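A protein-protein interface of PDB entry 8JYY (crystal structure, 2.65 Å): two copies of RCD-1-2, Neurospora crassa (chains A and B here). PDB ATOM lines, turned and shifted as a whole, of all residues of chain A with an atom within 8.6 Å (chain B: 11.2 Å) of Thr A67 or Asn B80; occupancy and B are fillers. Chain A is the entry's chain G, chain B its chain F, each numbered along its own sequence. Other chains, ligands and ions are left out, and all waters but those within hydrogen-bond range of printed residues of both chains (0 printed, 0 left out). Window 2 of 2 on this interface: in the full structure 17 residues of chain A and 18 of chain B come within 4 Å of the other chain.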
ATOM      1  N   ILE A  23       7.606  -7.004  10.335  1.00  0.00           N
ATOM      2  CA  ILE A  23       7.526  -5.891   9.386  1.00  0.00           C
ATOM      3  C   ILE A  23       8.010  -4.577   9.994  1.00  0.00           C
ATOM      4  O   ILE A  23       8.824  -3.891   9.353  1.00  0.00           O
ATOM      5  CB  ILE A  23       6.104  -5.792   8.805  1.00  0.00           C
ATOM      6  CG1 ILE A  23       5.930  -6.748   7.620  1.00  0.00           C
ATOM      7  CG2 ILE A  23       5.792  -4.363   8.379  1.00  0.00           C
ATOM      8  CD1 ILE A  23       5.784  -8.205   8.002  1.00  0.00           C
ATOM      9  N   MET A  26      12.105  -4.038  10.763  1.00  0.00           N
ATOM     10  CA  MET A  26      13.101  -3.921   9.703  1.00  0.00           C
ATOM     11  C   MET A  26      13.640  -2.498   9.607  1.00  0.00           C
ATOM     12  O   MET A  26      14.853  -2.290   9.497  1.00  0.00           O
ATOM     13  CB  MET A  26      12.504  -4.361   8.366  1.00  0.00           C
ATOM     14  CG  MET A  26      12.318  -5.862   8.226  1.00  0.00           C
ATOM     15  SD  MET A  26      11.822  -6.342   6.560  1.00  0.00           S
ATOM     16  CE  MET A  26      10.245  -5.503   6.421  1.00  0.00           C
ATOM     17  N   ILE A  37      17.352  -6.483   6.215  1.00  0.00           N
ATOM     18  CA  ILE A  37      17.870  -5.379   5.421  1.00  0.00           C
ATOM     19  C   ILE A  37      18.655  -4.436   6.320  1.00  0.00           C
ATOM     20  O   ILE A  37      18.197  -4.058   7.405  1.00  0.00           O
ATOM     21  CB  ILE A  37      16.721  -4.649   4.713  1.00  0.00           C
ATOM     22  CG1 ILE A  37      15.846  -5.643   3.948  1.00  0.00           C
ATOM     23  CG2 ILE A  37      17.269  -3.594   3.772  1.00  0.00           C
ATOM     24  CD1 ILE A  37      14.671  -5.000   3.246  1.00  0.00           C
ATOM     25  N   ASP A  64      12.314   3.604   1.940  1.00  0.00           N
ATOM     26  CA  ASP A  64      11.165   2.818   2.359  1.00  0.00           C
ATOM     27  C   ASP A  64      11.330   1.371   1.917  1.00  0.00           C
ATOM     28  O   ASP A  64      12.022   1.075   0.939  1.00  0.00           O
ATOM     29  CB  ASP A  64       9.862   3.386   1.785  1.00  0.00           C
ATOM     30  CG  ASP A  64       9.444   4.681   2.454  1.00  0.00           C
ATOM     31  OD1 ASP A  64       9.816   4.893   3.628  1.00  0.00           O
ATOM     32  OD2 ASP A  64       8.739   5.484   1.808  1.00  0.00           O
ATOM     33  N   VAL A  65      10.682   0.470   2.648  1.00  0.00           N
ATOM     34  CA  VAL A  65      10.698  -0.953   2.328  1.00  0.00           C
ATOM     35  C   VAL A  65       9.600  -1.232   1.310  1.00  0.00           C
ATOM     36  O   VAL A  65       8.410  -1.068   1.601  1.00  0.00           O
ATOM     37  CB  VAL A  65      10.524  -1.810   3.589  1.00  0.00           C
ATOM     38  CG1 VAL A  65      11.846  -1.929   4.327  1.00  0.00           C
ATOM     39  CG2 VAL A  65       9.470  -1.208   4.509  1.00  0.00           C
ATOM     40  N   PHE A  66       9.997  -1.640   0.109  1.00  0.00           N
ATOM     41  CA  PHE A  66       9.060  -1.952  -0.959  1.00  0.00           C
ATOM     42  C   PHE A  66       8.904  -3.461  -1.087  1.00  0.00           C
ATOM     43  O   PHE A  66       9.877  -4.212  -0.964  1.00  0.00           O
ATOM     44  CB  PHE A  66       9.523  -1.345  -2.285  1.00  0.00           C
ATOM     45  CG  PHE A  66       9.561   0.156  -2.276  1.00  0.00           C
ATOM     46  CD1 PHE A  66       8.416   0.892  -2.532  1.00  0.00           C
ATOM     47  CD2 PHE A  66      10.737   0.832  -2.002  1.00  0.00           C
ATOM     48  CE1 PHE A  66       8.445   2.276  -2.519  1.00  0.00           C
ATOM     49  CE2 PHE A  66      10.774   2.215  -1.989  1.00  0.00           C
ATOM     50  CZ  PHE A  66       9.626   2.937  -2.248  1.00  0.00           C
ATOM     51  N   THR A  67       7.674  -3.902  -1.332  1.00  0.00           N
ATOM     52  CA  THR A  67       7.330  -5.313  -1.301  1.00  0.00           C
ATOM     53  C   THR A  67       6.994  -5.829  -2.693  1.00  0.00           C
ATOM     54  O   THR A  67       6.612  -5.075  -3.592  1.00  0.00           O
ATOM     55  CB  THR A  67       6.146  -5.568  -0.361  1.00  0.00           C
ATOM     56  OG1 THR A  67       4.986  -4.888  -0.859  1.00  0.00           O
ATOM     57  CG2 THR A  67       6.460  -5.063   1.039  1.00  0.00           C
ATOM     58  N   ALA A  68       7.151  -7.140  -2.856  1.00  0.00           N
ATOM     59  CA  ALA A  68       6.735  -7.824  -4.079  1.00  0.00           C
ATOM     60  C   ALA A  68       6.298  -9.235  -3.717  1.00  0.00           C
ATOM     61  O   ALA A  68       7.080  -9.993  -3.138  1.00  0.00           O
ATOM     62  CB  ALA A  68       7.863  -7.851  -5.111  1.00  0.00           C
ATOM     63  N   HIS A  69       5.062  -9.589  -4.057  1.00  0.00           N
ATOM     64  CA  HIS A  69       4.498 -10.883  -3.693  1.00  0.00           C
ATOM     65  C   HIS A  69       4.502 -11.829  -4.887  1.00  0.00           C
ATOM     66  O   HIS A  69       4.242 -11.417  -6.021  1.00  0.00           O
ATOM     67  CB  HIS A  69       3.071 -10.726  -3.158  1.00  0.00           C
ATOM     68  CG  HIS A  69       2.976  -9.880  -1.927  1.00  0.00           C
ATOM     69  ND1 HIS A  69       3.152  -8.513  -1.948  1.00  0.00           N
ATOM     70  CD2 HIS A  69       2.730 -10.207  -0.636  1.00  0.00           C
ATOM     71  CE1 HIS A  69       3.014  -8.034  -0.725  1.00  0.00           C
ATOM     72  NE2 HIS A  69       2.759  -9.042   0.091  1.00  0.00           N
ATOM     73  N   TYR A  70       4.797 -13.102  -4.622  1.00  0.00           N
ATOM     74  CA  TYR A  70       4.789 -14.145  -5.635  1.00  0.00           C
ATOM     75  C   TYR A  70       4.115 -15.380  -5.054  1.00  0.00           C
ATOM     76  O   TYR A  70       4.160 -15.616  -3.843  1.00  0.00           O
ATOM     77  CB  TYR A  70       6.208 -14.494  -6.109  1.00  0.00           C
ATOM     78  CG  TYR A  70       7.020 -13.323  -6.621  1.00  0.00           C
ATOM     79  CD1 TYR A  70       7.679 -12.471  -5.743  1.00  0.00           C
ATOM     80  CD2 TYR A  70       7.144 -13.082  -7.983  1.00  0.00           C
ATOM     81  CE1 TYR A  70       8.426 -11.404  -6.206  1.00  0.00           C
ATOM     82  CE2 TYR A  70       7.891 -12.018  -8.456  1.00  0.00           C
ATOM     83  CZ  TYR A  70       8.528 -11.183  -7.563  1.00  0.00           C
ATOM     84  OH  TYR A  70       9.271 -10.125  -8.032  1.00  0.00           O
ATOM     85  N   VAL A 104       5.926 -16.213  -1.610  1.00  0.00           N
ATOM     86  CA  VAL A 104       7.235 -15.641  -1.323  1.00  0.00           C
ATOM     87  C   VAL A 104       7.137 -14.128  -1.459  1.00  0.00           C
ATOM     88  O   VAL A 104       6.663 -13.621  -2.481  1.00  0.00           O
ATOM     89  CB  VAL A 104       8.327 -16.197  -2.256  1.00  0.00           C
ATOM     90  CG1 VAL A 104       9.638 -15.472  -2.017  1.00  0.00           C
ATOM     91  CG2 VAL A 104       8.501 -17.689  -2.037  1.00  0.00           C
ATOM     92  N   VAL A 105       7.587 -13.411  -0.435  1.00  0.00           N
ATOM     93  CA  VAL A 105       7.531 -11.957  -0.411  1.00  0.00           C
ATOM     94  C   VAL A 105       8.952 -11.414  -0.392  1.00  0.00           C
ATOM     95  O   VAL A 105       9.757 -11.792   0.469  1.00  0.00           O
ATOM     96  CB  VAL A 105       6.730 -11.435   0.797  1.00  0.00           C
ATOM     97  CG1 VAL A 105       6.619  -9.920   0.740  1.00  0.00           C
ATOM     98  CG2 VAL A 105       5.351 -12.079   0.834  1.00  0.00           C
ATOM     99  N   GLU A 106       9.256 -10.542  -1.351  1.00  0.00           N
ATOM    100  CA  GLU A 106      10.508  -9.801  -1.376  1.00  0.00           C
ATOM    101  C   GLU A 106      10.306  -8.457  -0.694  1.00  0.00           C
ATOM    102  O   GLU A 106       9.355  -7.733  -1.011  1.00  0.00           O
ATOM    103  CB  GLU A 106      10.990  -9.570  -2.809  1.00  0.00           C
ATOM    104  CG  GLU A 106      11.035 -10.795  -3.693  1.00  0.00           C
ATOM    105  CD  GLU A 106      11.710 -10.516  -5.023  1.00  0.00           C
ATOM    106  OE1 GLU A 106      11.997  -9.333  -5.310  1.00  0.00           O
ATOM    107  OE2 GLU A 106      11.958 -11.478  -5.779  1.00  0.00           O
ATOM    108  N   TYR A 107      11.198  -8.133   0.237  1.00  0.00           N
ATOM    109  CA  TYR A 107      11.301  -6.804   0.823  1.00  0.00           C
ATOM    110  C   TYR A 107      12.627  -6.211   0.376  1.00  0.00           C
ATOM    111  O   TYR A 107      13.686  -6.812   0.600  1.00  0.00           O
ATOM    112  CB  TYR A 107      11.220  -6.858   2.348  1.00  0.00           C
ATOM    113  CG  TYR A 107       9.994  -7.563   2.872  1.00  0.00           C
ATOM    114  CD1 TYR A 107       8.792  -6.887   3.029  1.00  0.00           C
ATOM    115  CD2 TYR A 107      10.037  -8.908   3.213  1.00  0.00           C
ATOM    116  CE1 TYR A 107       7.667  -7.530   3.509  1.00  0.00           C
ATOM    117  CE2 TYR A 107       8.921  -9.556   3.694  1.00  0.00           C
ATOM    118  CZ  TYR A 107       7.737  -8.866   3.841  1.00  0.00           C
ATOM    119  OH  TYR A 107       6.623  -9.517   4.319  1.00  0.00           O
ATOM    120  N   ALA A 108      12.572  -5.043  -0.261  1.00  0.00           N
ATOM    121  CA  ALA A 108      13.746  -4.431  -0.861  1.00  0.00           C
ATOM    122  C   ALA A 108      13.812  -2.953  -0.510  1.00  0.00           C
ATOM    123  O   ALA A 108      12.790  -2.307  -0.266  1.00  0.00           O
ATOM    124  CB  ALA A 108      13.746  -4.601  -2.386  1.00  0.00           C
ATOM    125  N   VAL A 109      15.038  -2.426  -0.491  1.00  0.00           N
ATOM    126  CA  VAL A 109      15.292  -1.010  -0.267  1.00  0.00           C
ATOM    127  C   VAL A 109      16.443  -0.588  -1.169  1.00  0.00           C
ATOM    128  O   VAL A 109      17.224  -1.414  -1.647  1.00  0.00           O
ATOM    129  CB  VAL A 109      15.620  -0.694   1.212  1.00  0.00           C
ATOM    130  CG1 VAL A 109      17.109  -0.877   1.482  1.00  0.00           C
ATOM    131  CG2 VAL A 109      15.171   0.714   1.574  1.00  0.00           C
ATOM    132  N   ILE A 147      15.506  -9.005   1.247  1.00  0.00           N
ATOM    133  CA  ILE A 147      15.277 -10.319   1.839  1.00  0.00           C
ATOM    134  C   ILE A 147      14.012 -10.930   1.251  1.00  0.00           C
ATOM    135  O   ILE A 147      13.011 -10.239   1.035  1.00  0.00           O
ATOM    136  CB  ILE A 147      15.178 -10.260   3.381  1.00  0.00           C
ATOM    137  CG1 ILE A 147      14.116  -9.253   3.825  1.00  0.00           C
ATOM    138  CG2 ILE A 147      16.533  -9.941   3.997  1.00  0.00           C
ATOM    139  CD1 ILE A 147      13.837  -9.283   5.313  1.00  0.00           C
ATOM    140  N   GLY B   2       4.753 -18.021  -9.784  1.00  0.00           N
ATOM    141  CA  GLY B   2       6.163 -17.781  -9.550  1.00  0.00           C
ATOM    142  C   GLY B   2       6.623 -16.486 -10.190  1.00  0.00           C
ATOM    143  O   GLY B   2       5.892 -15.492 -10.258  1.00  0.00           O
ATOM    144  N   ARG B   3       7.863 -16.497 -10.670  1.00  0.00           N
ATOM    145  CA  ARG B   3       8.389 -15.335 -11.372  1.00  0.00           C
ATOM    146  C   ARG B   3       7.875 -15.323 -12.811  1.00  0.00           C
ATOM    147  O   ARG B   3       7.830 -16.371 -13.461  1.00  0.00           O
ATOM    148  CB  ARG B   3       9.916 -15.345 -11.359  1.00  0.00           C
ATOM    149  CG  ARG B   3      10.539 -13.999 -11.035  1.00  0.00           C
ATOM    150  CD  ARG B   3      11.696 -14.151 -10.063  1.00  0.00           C
ATOM    151  NE  ARG B   3      12.040 -12.884  -9.430  1.00  0.00           N
ATOM    152  CZ  ARG B   3      12.851 -12.765  -8.387  1.00  0.00           C
ATOM    153  NH1 ARG B   3      13.420 -13.822  -7.831  1.00  0.00           N
ATOM    154  NH2 ARG B   3      13.095 -11.556  -7.890  1.00  0.00           N
ATOM    155  N   HIS B  74       2.991 -17.584 -16.158  1.00  0.00           N
ATOM    156  CA  HIS B  74       2.142 -16.429 -16.398  1.00  0.00           C
ATOM    157  C   HIS B  74       2.969 -15.315 -17.022  1.00  0.00           C
ATOM    158  O   HIS B  74       4.200 -15.303 -16.942  1.00  0.00           O
ATOM    159  CB  HIS B  74       1.462 -15.944 -15.110  1.00  0.00           C
ATOM    160  CG  HIS B  74       2.384 -15.248 -14.158  1.00  0.00           C
ATOM    161  ND1 HIS B  74       3.280 -15.925 -13.360  1.00  0.00           N
ATOM    162  CD2 HIS B  74       2.541 -13.935 -13.869  1.00  0.00           C
ATOM    163  CE1 HIS B  74       3.952 -15.059 -12.623  1.00  0.00           C
ATOM    164  NE2 HIS B  74       3.523 -13.844 -12.914  1.00  0.00           N
ATOM    165  N   GLY B  76       3.279 -11.120 -17.346  1.00  0.00           N
ATOM    166  CA  GLY B  76       2.961  -9.761 -16.958  1.00  0.00           C
ATOM    167  C   GLY B  76       3.120  -9.528 -15.465  1.00  0.00           C
ATOM    168  O   GLY B  76       3.246 -10.452 -14.663  1.00  0.00           O
ATOM    169  N   ASP B  77       3.111  -8.245 -15.114  1.00  0.00           N
ATOM    170  CA  ASP B  77       3.177  -7.789 -13.734  1.00  0.00           C
ATOM    171  C   ASP B  77       1.796  -7.350 -13.257  1.00  0.00           C
ATOM    172  O   ASP B  77       0.843  -7.245 -14.032  1.00  0.00           O
ATOM    173  CB  ASP B  77       4.189  -6.648 -13.592  1.00  0.00           C
ATOM    174  CG  ASP B  77       4.089  -5.635 -14.716  1.00  0.00           C
ATOM    175  OD1 ASP B  77       3.916  -6.054 -15.881  1.00  0.00           O
ATOM    176  OD2 ASP B  77       4.181  -4.421 -14.437  1.00  0.00           O
ATOM    177  N   HIS B  78       1.695  -7.091 -11.956  1.00  0.00           N
ATOM    178  CA  HIS B  78       0.424  -6.798 -11.303  1.00  0.00           C
ATOM    179  C   HIS B  78       0.415  -5.368 -10.771  1.00  0.00           C
ATOM    180  O   HIS B  78       1.353  -4.593 -10.973  1.00  0.00           O
ATOM    181  CB  HIS B  78       0.149  -7.795 -10.173  1.00  0.00           C
ATOM    182  CG  HIS B  78      -0.036  -9.204 -10.642  1.00  0.00           C
ATOM    183  ND1 HIS B  78       0.078  -9.568 -11.967  1.00  0.00           N
ATOM    184  CD2 HIS B  78      -0.330 -10.338  -9.964  1.00  0.00           C
ATOM    185  CE1 HIS B  78      -0.133 -10.866 -12.084  1.00  0.00           C
ATOM    186  NE2 HIS B  78      -0.385 -11.358 -10.883  1.00  0.00           N
ATOM    187  N   LEU B  79      -0.671  -5.027 -10.075  1.00  0.00           N
ATOM    188  CA  LEU B  79      -0.854  -3.698  -9.509  1.00  0.00           C
ATOM    189  C   LEU B  79      -0.135  -3.510  -8.180  1.00  0.00           C
ATOM    190  O   LEU B  79      -0.261  -2.440  -7.574  1.00  0.00           O
ATOM    191  CB  LEU B  79      -2.349  -3.398  -9.339  1.00  0.00           C
ATOM    192  CG  LEU B  79      -3.211  -4.350  -8.503  1.00  0.00           C
ATOM    193  CD1 LEU B  79      -3.233  -3.955  -7.028  1.00  0.00           C
ATOM    194  CD2 LEU B  79      -4.626  -4.415  -9.061  1.00  0.00           C
ATOM    195  N   ASN B  80       0.603  -4.518  -7.705  1.00  0.00           N
ATOM    196  CA  ASN B  80       1.401  -4.338  -6.499  1.00  0.00           C
ATOM    197  C   ASN B  80       2.497  -3.304  -6.717  1.00  0.00           C
ATOM    198  O   ASN B  80       2.956  -2.669  -5.760  1.00  0.00           O
ATOM    199  CB  ASN B  80       1.999  -5.678  -6.059  1.00  0.00           C
ATOM    200  CG  ASN B  80       2.588  -5.628  -4.659  1.00  0.00           C
ATOM    201  OD1 ASN B  80       2.335  -4.695  -3.897  1.00  0.00           O
ATOM    202  ND2 ASN B  80       3.372  -6.643  -4.312  1.00  0.00           N
ATOM    203  N   SER B  81       2.923  -3.116  -7.968  1.00  0.00           N
ATOM    204  CA  SER B  81       3.914  -2.094  -8.281  1.00  0.00           C
ATOM    205  C   SER B  81       3.270  -0.716  -8.388  1.00  0.00           C
ATOM    206  O   SER B  81       3.783   0.258  -7.832  1.00  0.00           O
ATOM    207  CB  SER B  81       4.642  -2.450  -9.578  1.00  0.00           C
ATOM    208  OG  SER B  81       5.599  -1.461  -9.919  1.00  0.00           O
ATOM    209  N   GLU B  82       2.136  -0.624  -9.089  1.00  0.00           N
ATOM    210  CA  GLU B  82       1.483   0.664  -9.309  1.00  0.00           C
ATOM    211  C   GLU B  82       1.082   1.345  -8.008  1.00  0.00           C
ATOM    212  O   GLU B  82       0.941   2.573  -7.982  1.00  0.00           O
ATOM    213  CB  GLU B  82       0.255   0.476 -10.202  1.00  0.00           C
ATOM    214  CG  GLU B  82       0.561  -0.221 -11.519  1.00  0.00           C
ATOM    215  CD  GLU B  82      -0.680  -0.771 -12.200  1.00  0.00           C
ATOM    216  OE1 GLU B  82      -1.711  -0.066 -12.230  1.00  0.00           O
ATOM    217  OE2 GLU B  82      -0.623  -1.915 -12.698  1.00  0.00           O
ATOM    218  N   PHE B  83       0.900   0.584  -6.929  1.00  0.00           N
ATOM    219  CA  PHE B  83       0.552   1.185  -5.647  1.00  0.00           C
ATOM    220  C   PHE B  83       1.787   1.741  -4.943  1.00  0.00           C
ATOM    221  O   PHE B  83       1.767   2.872  -4.442  1.00  0.00           O
ATOM    222  CB  PHE B  83      -0.162   0.155  -4.769  1.00  0.00           C
ATOM    223  CG  PHE B  83      -0.323   0.580  -3.337  1.00  0.00           C
ATOM    224  CD1 PHE B  83      -1.205   1.592  -2.990  1.00  0.00           C
ATOM    225  CD2 PHE B  83       0.397  -0.046  -2.335  1.00  0.00           C
ATOM    226  CE1 PHE B  83      -1.355   1.977  -1.670  1.00  0.00           C
ATOM    227  CE2 PHE B  83       0.251   0.333  -1.013  1.00  0.00           C
ATOM    228  CZ  PHE B  83      -0.626   1.346  -0.680  1.00  0.00           C
ATOM    229  N   VAL B  84       2.877   0.968  -4.911  1.00  0.00           N
ATOM    230  CA  VAL B  84       4.099   1.361  -4.214  1.00  0.00           C
ATOM    231  C   VAL B  84       4.860   2.357  -5.075  1.00  0.00           C
ATOM    232  O   VAL B  84       5.907   2.873  -4.666  1.00  0.00           O
ATOM    233  CB  VAL B  84       4.981   0.144  -3.874  1.00  0.00           C
ATOM    234  CG1 VAL B  84       4.245  -0.830  -2.955  1.00  0.00           C
ATOM    235  CG2 VAL B  84       5.437  -0.554  -5.147  1.00  0.00           C
ATOM    236  N   VAL B  85       4.344   2.633  -6.270  1.00  0.00           N
ATOM    237  CA  VAL B  85       4.988   3.558  -7.194  1.00  0.00           C
ATOM    238  C   VAL B  85       4.225   4.872  -7.345  1.00  0.00           C
ATOM    239  O   VAL B  85       4.850   5.893  -7.677  1.00  0.00           O
ATOM    240  CB  VAL B  85       5.205   2.887  -8.571  1.00  0.00           C
ATOM    241  CG1 VAL B  85       4.775   3.778  -9.718  1.00  0.00           C
ATOM    242  CG2 VAL B  85       6.651   2.475  -8.735  1.00  0.00           C
ATOM    243  N   GLN B  86       2.921   4.893  -7.059  1.00  0.00           N
ATOM    244  CA  GLN B  86       2.040   6.025  -7.362  1.00  0.00           C
ATOM    245  C   GLN B  86       1.935   6.231  -8.872  1.00  0.00           C
ATOM    246  O   GLN B  86       2.120   7.334  -9.394  1.00  0.00           O
ATOM    247  CB  GLN B  86       2.489   7.309  -6.654  1.00  0.00           C
ATOM    248  CG  GLN B  86       2.314   7.282  -5.144  1.00  0.00           C
ATOM    249  CD  GLN B  86       0.876   7.049  -4.724  1.00  0.00           C
ATOM    250  OE1 GLN B  86      -0.043   7.704  -5.217  1.00  0.00           O
ATOM    251  NE2 GLN B  86       0.673   6.107  -3.810  1.00  0.00           N
ATOM    252  N   ALA B  87       1.641   5.143  -9.577  1.00  0.00           N
ATOM    253  CA  ALA B  87       1.358   5.192 -11.000  1.00  0.00           C
ATOM    254  C   ALA B  87      -0.139   5.382 -11.231  1.00  0.00           C
ATOM    255  O   ALA B  87      -0.957   5.274 -10.315  1.00  0.00           O
ATOM    256  CB  ALA B  87       1.850   3.923 -11.696  1.00  0.00           C
ATOM    257  N   GLY B  88      -0.492   5.667 -12.481  1.00  0.00           N
ATOM    258  CA  GLY B  88      -1.884   5.905 -12.811  1.00  0.00           C
ATOM    259  C   GLY B  88      -2.717   4.642 -12.668  1.00  0.00           C
ATOM    260  O   GLY B  88      -2.285   3.541 -13.010  1.00  0.00           O
ATOM    261  N   LEU B  89      -3.934   4.814 -12.146  1.00  0.00           N
ATOM    262  CA  LEU B  89      -4.870   3.703 -12.037  1.00  0.00           C
ATOM    263  C   LEU B  89      -5.389   3.242 -13.392  1.00  0.00           C
ATOM    264  O   LEU B  89      -6.070   2.213 -13.458  1.00  0.00           O
ATOM    265  CB  LEU B  89      -6.045   4.096 -11.139  1.00  0.00           C
ATOM    266  CG  LEU B  89      -5.699   4.518  -9.710  1.00  0.00           C
ATOM    267  CD1 LEU B  89      -6.956   4.912  -8.948  1.00  0.00           C
ATOM    268  CD2 LEU B  89      -4.955   3.406  -8.985  1.00  0.00           C
ATOM    269  N   ASP B  97      -5.558  -9.500 -14.275  1.00  0.00           N
ATOM    270  CA  ASP B  97      -5.659  -9.599 -15.727  1.00  0.00           C
ATOM    271  C   ASP B  97      -4.322 -10.006 -16.339  1.00  0.00           C
ATOM    272  O   ASP B  97      -3.538  -9.156 -16.763  1.00  0.00           O
ATOM    273  CB  ASP B  97      -6.136  -8.273 -16.322  1.00  0.00           C
ATOM    274  CG  ASP B  97      -6.285  -8.330 -17.830  1.00  0.00           C
ATOM    275  OD1 ASP B  97      -7.148  -9.091 -18.316  1.00  0.00           O
ATOM    276  OD2 ASP B  97      -5.539  -7.613 -18.530  1.00  0.00           O
ATOM    277  N   ARG B  98      -4.066 -11.312 -16.383  1.00  0.00           N
ATOM    278  CA  ARG B  98      -2.824 -11.836 -16.929  1.00  0.00           C
ATOM    279  C   ARG B  98      -3.112 -13.112 -17.707  1.00  0.00           C
ATOM    280  O   ARG B  98      -4.174 -13.725 -17.569  1.00  0.00           O
ATOM    281  CB  ARG B  98      -1.791 -12.113 -15.826  1.00  0.00           C
ATOM    282  CG  ARG B  98      -2.175 -13.245 -14.882  1.00  0.00           C
ATOM    283  CD  ARG B  98      -1.073 -13.509 -13.868  1.00  0.00           C
ATOM    284  NE  ARG B  98      -1.422 -14.563 -12.923  1.00  0.00           N
ATOM    285  CZ  ARG B  98      -0.695 -14.886 -11.862  1.00  0.00           C
ATOM    286  NH1 ARG B  98       0.422 -14.241 -11.566  1.00  0.00           N
ATOM    287  NH2 ARG B  98      -1.099 -15.880 -11.075  1.00  0.00           N
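Among the printed residues, merely in contact across the chains: Phe A66 with Val B84, Thr A67 with Asn B80, Ala A68 with Asn B80 and Tyr A70 with Gly B2.
Hydrophobic or aromatic side chains of chain B within 4 Å of the printed part of chain A: Val B84. Among the printed residues, 6 pairs touch across the chains. Among the printed residues, Asp or Glu carboxylates within 4 Å of a Lys or Arg side-chain nitrogen of the other chain: Glu A106 with Arg B3.
No position is printed for both chains.
The backbone NH (N) of Tyr A70 sits at hydrogen-bond distance from the backbone carbonyl oxygen (O) of Val A104 (2.9 Å). The backbone NH of Phe A66 lies within hydrogen-bond range of the backbone carbonyl oxygen of Ala A108 (2.9 Å). The backbone carbonyl oxygen of Ala A68 sits at hydrogen-bond distance from the backbone NH of Glu A106, 2.9 Å away.
Printed residues of chain B within 4 Å of Phe A66: Val B84. Thr A67 touches just one residue of chain B: Asn B80. Ala A68 touches one residue of chain B. Printed residues of chain B within 4 Å of His A69: Asn B80. Of the printed residues of chain B, Glu A106 touches Arg B3 (2.4 Å). No residue of chain B comes within 4 Å of Tyr A107. No residue of chain B comes within 4 Å of Ala A108. Of chain A, only Thr A67 (3.7 Å), Ala A68 (3.6 Å) and His A69 (3.0 Å) come within 4 Å of Asn B80. The nearest printed residue of chain A that does not touch Gly B2 is His A69 (6.1 Å).
NH1 of Arg B3 lies within salt-bridge range of OE2 of Glu A106. A ring nitrogen (ND1) of His A69 is in hydrogen-bond range of the side-chain amide nitrogen (ND2) of Asn B80.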
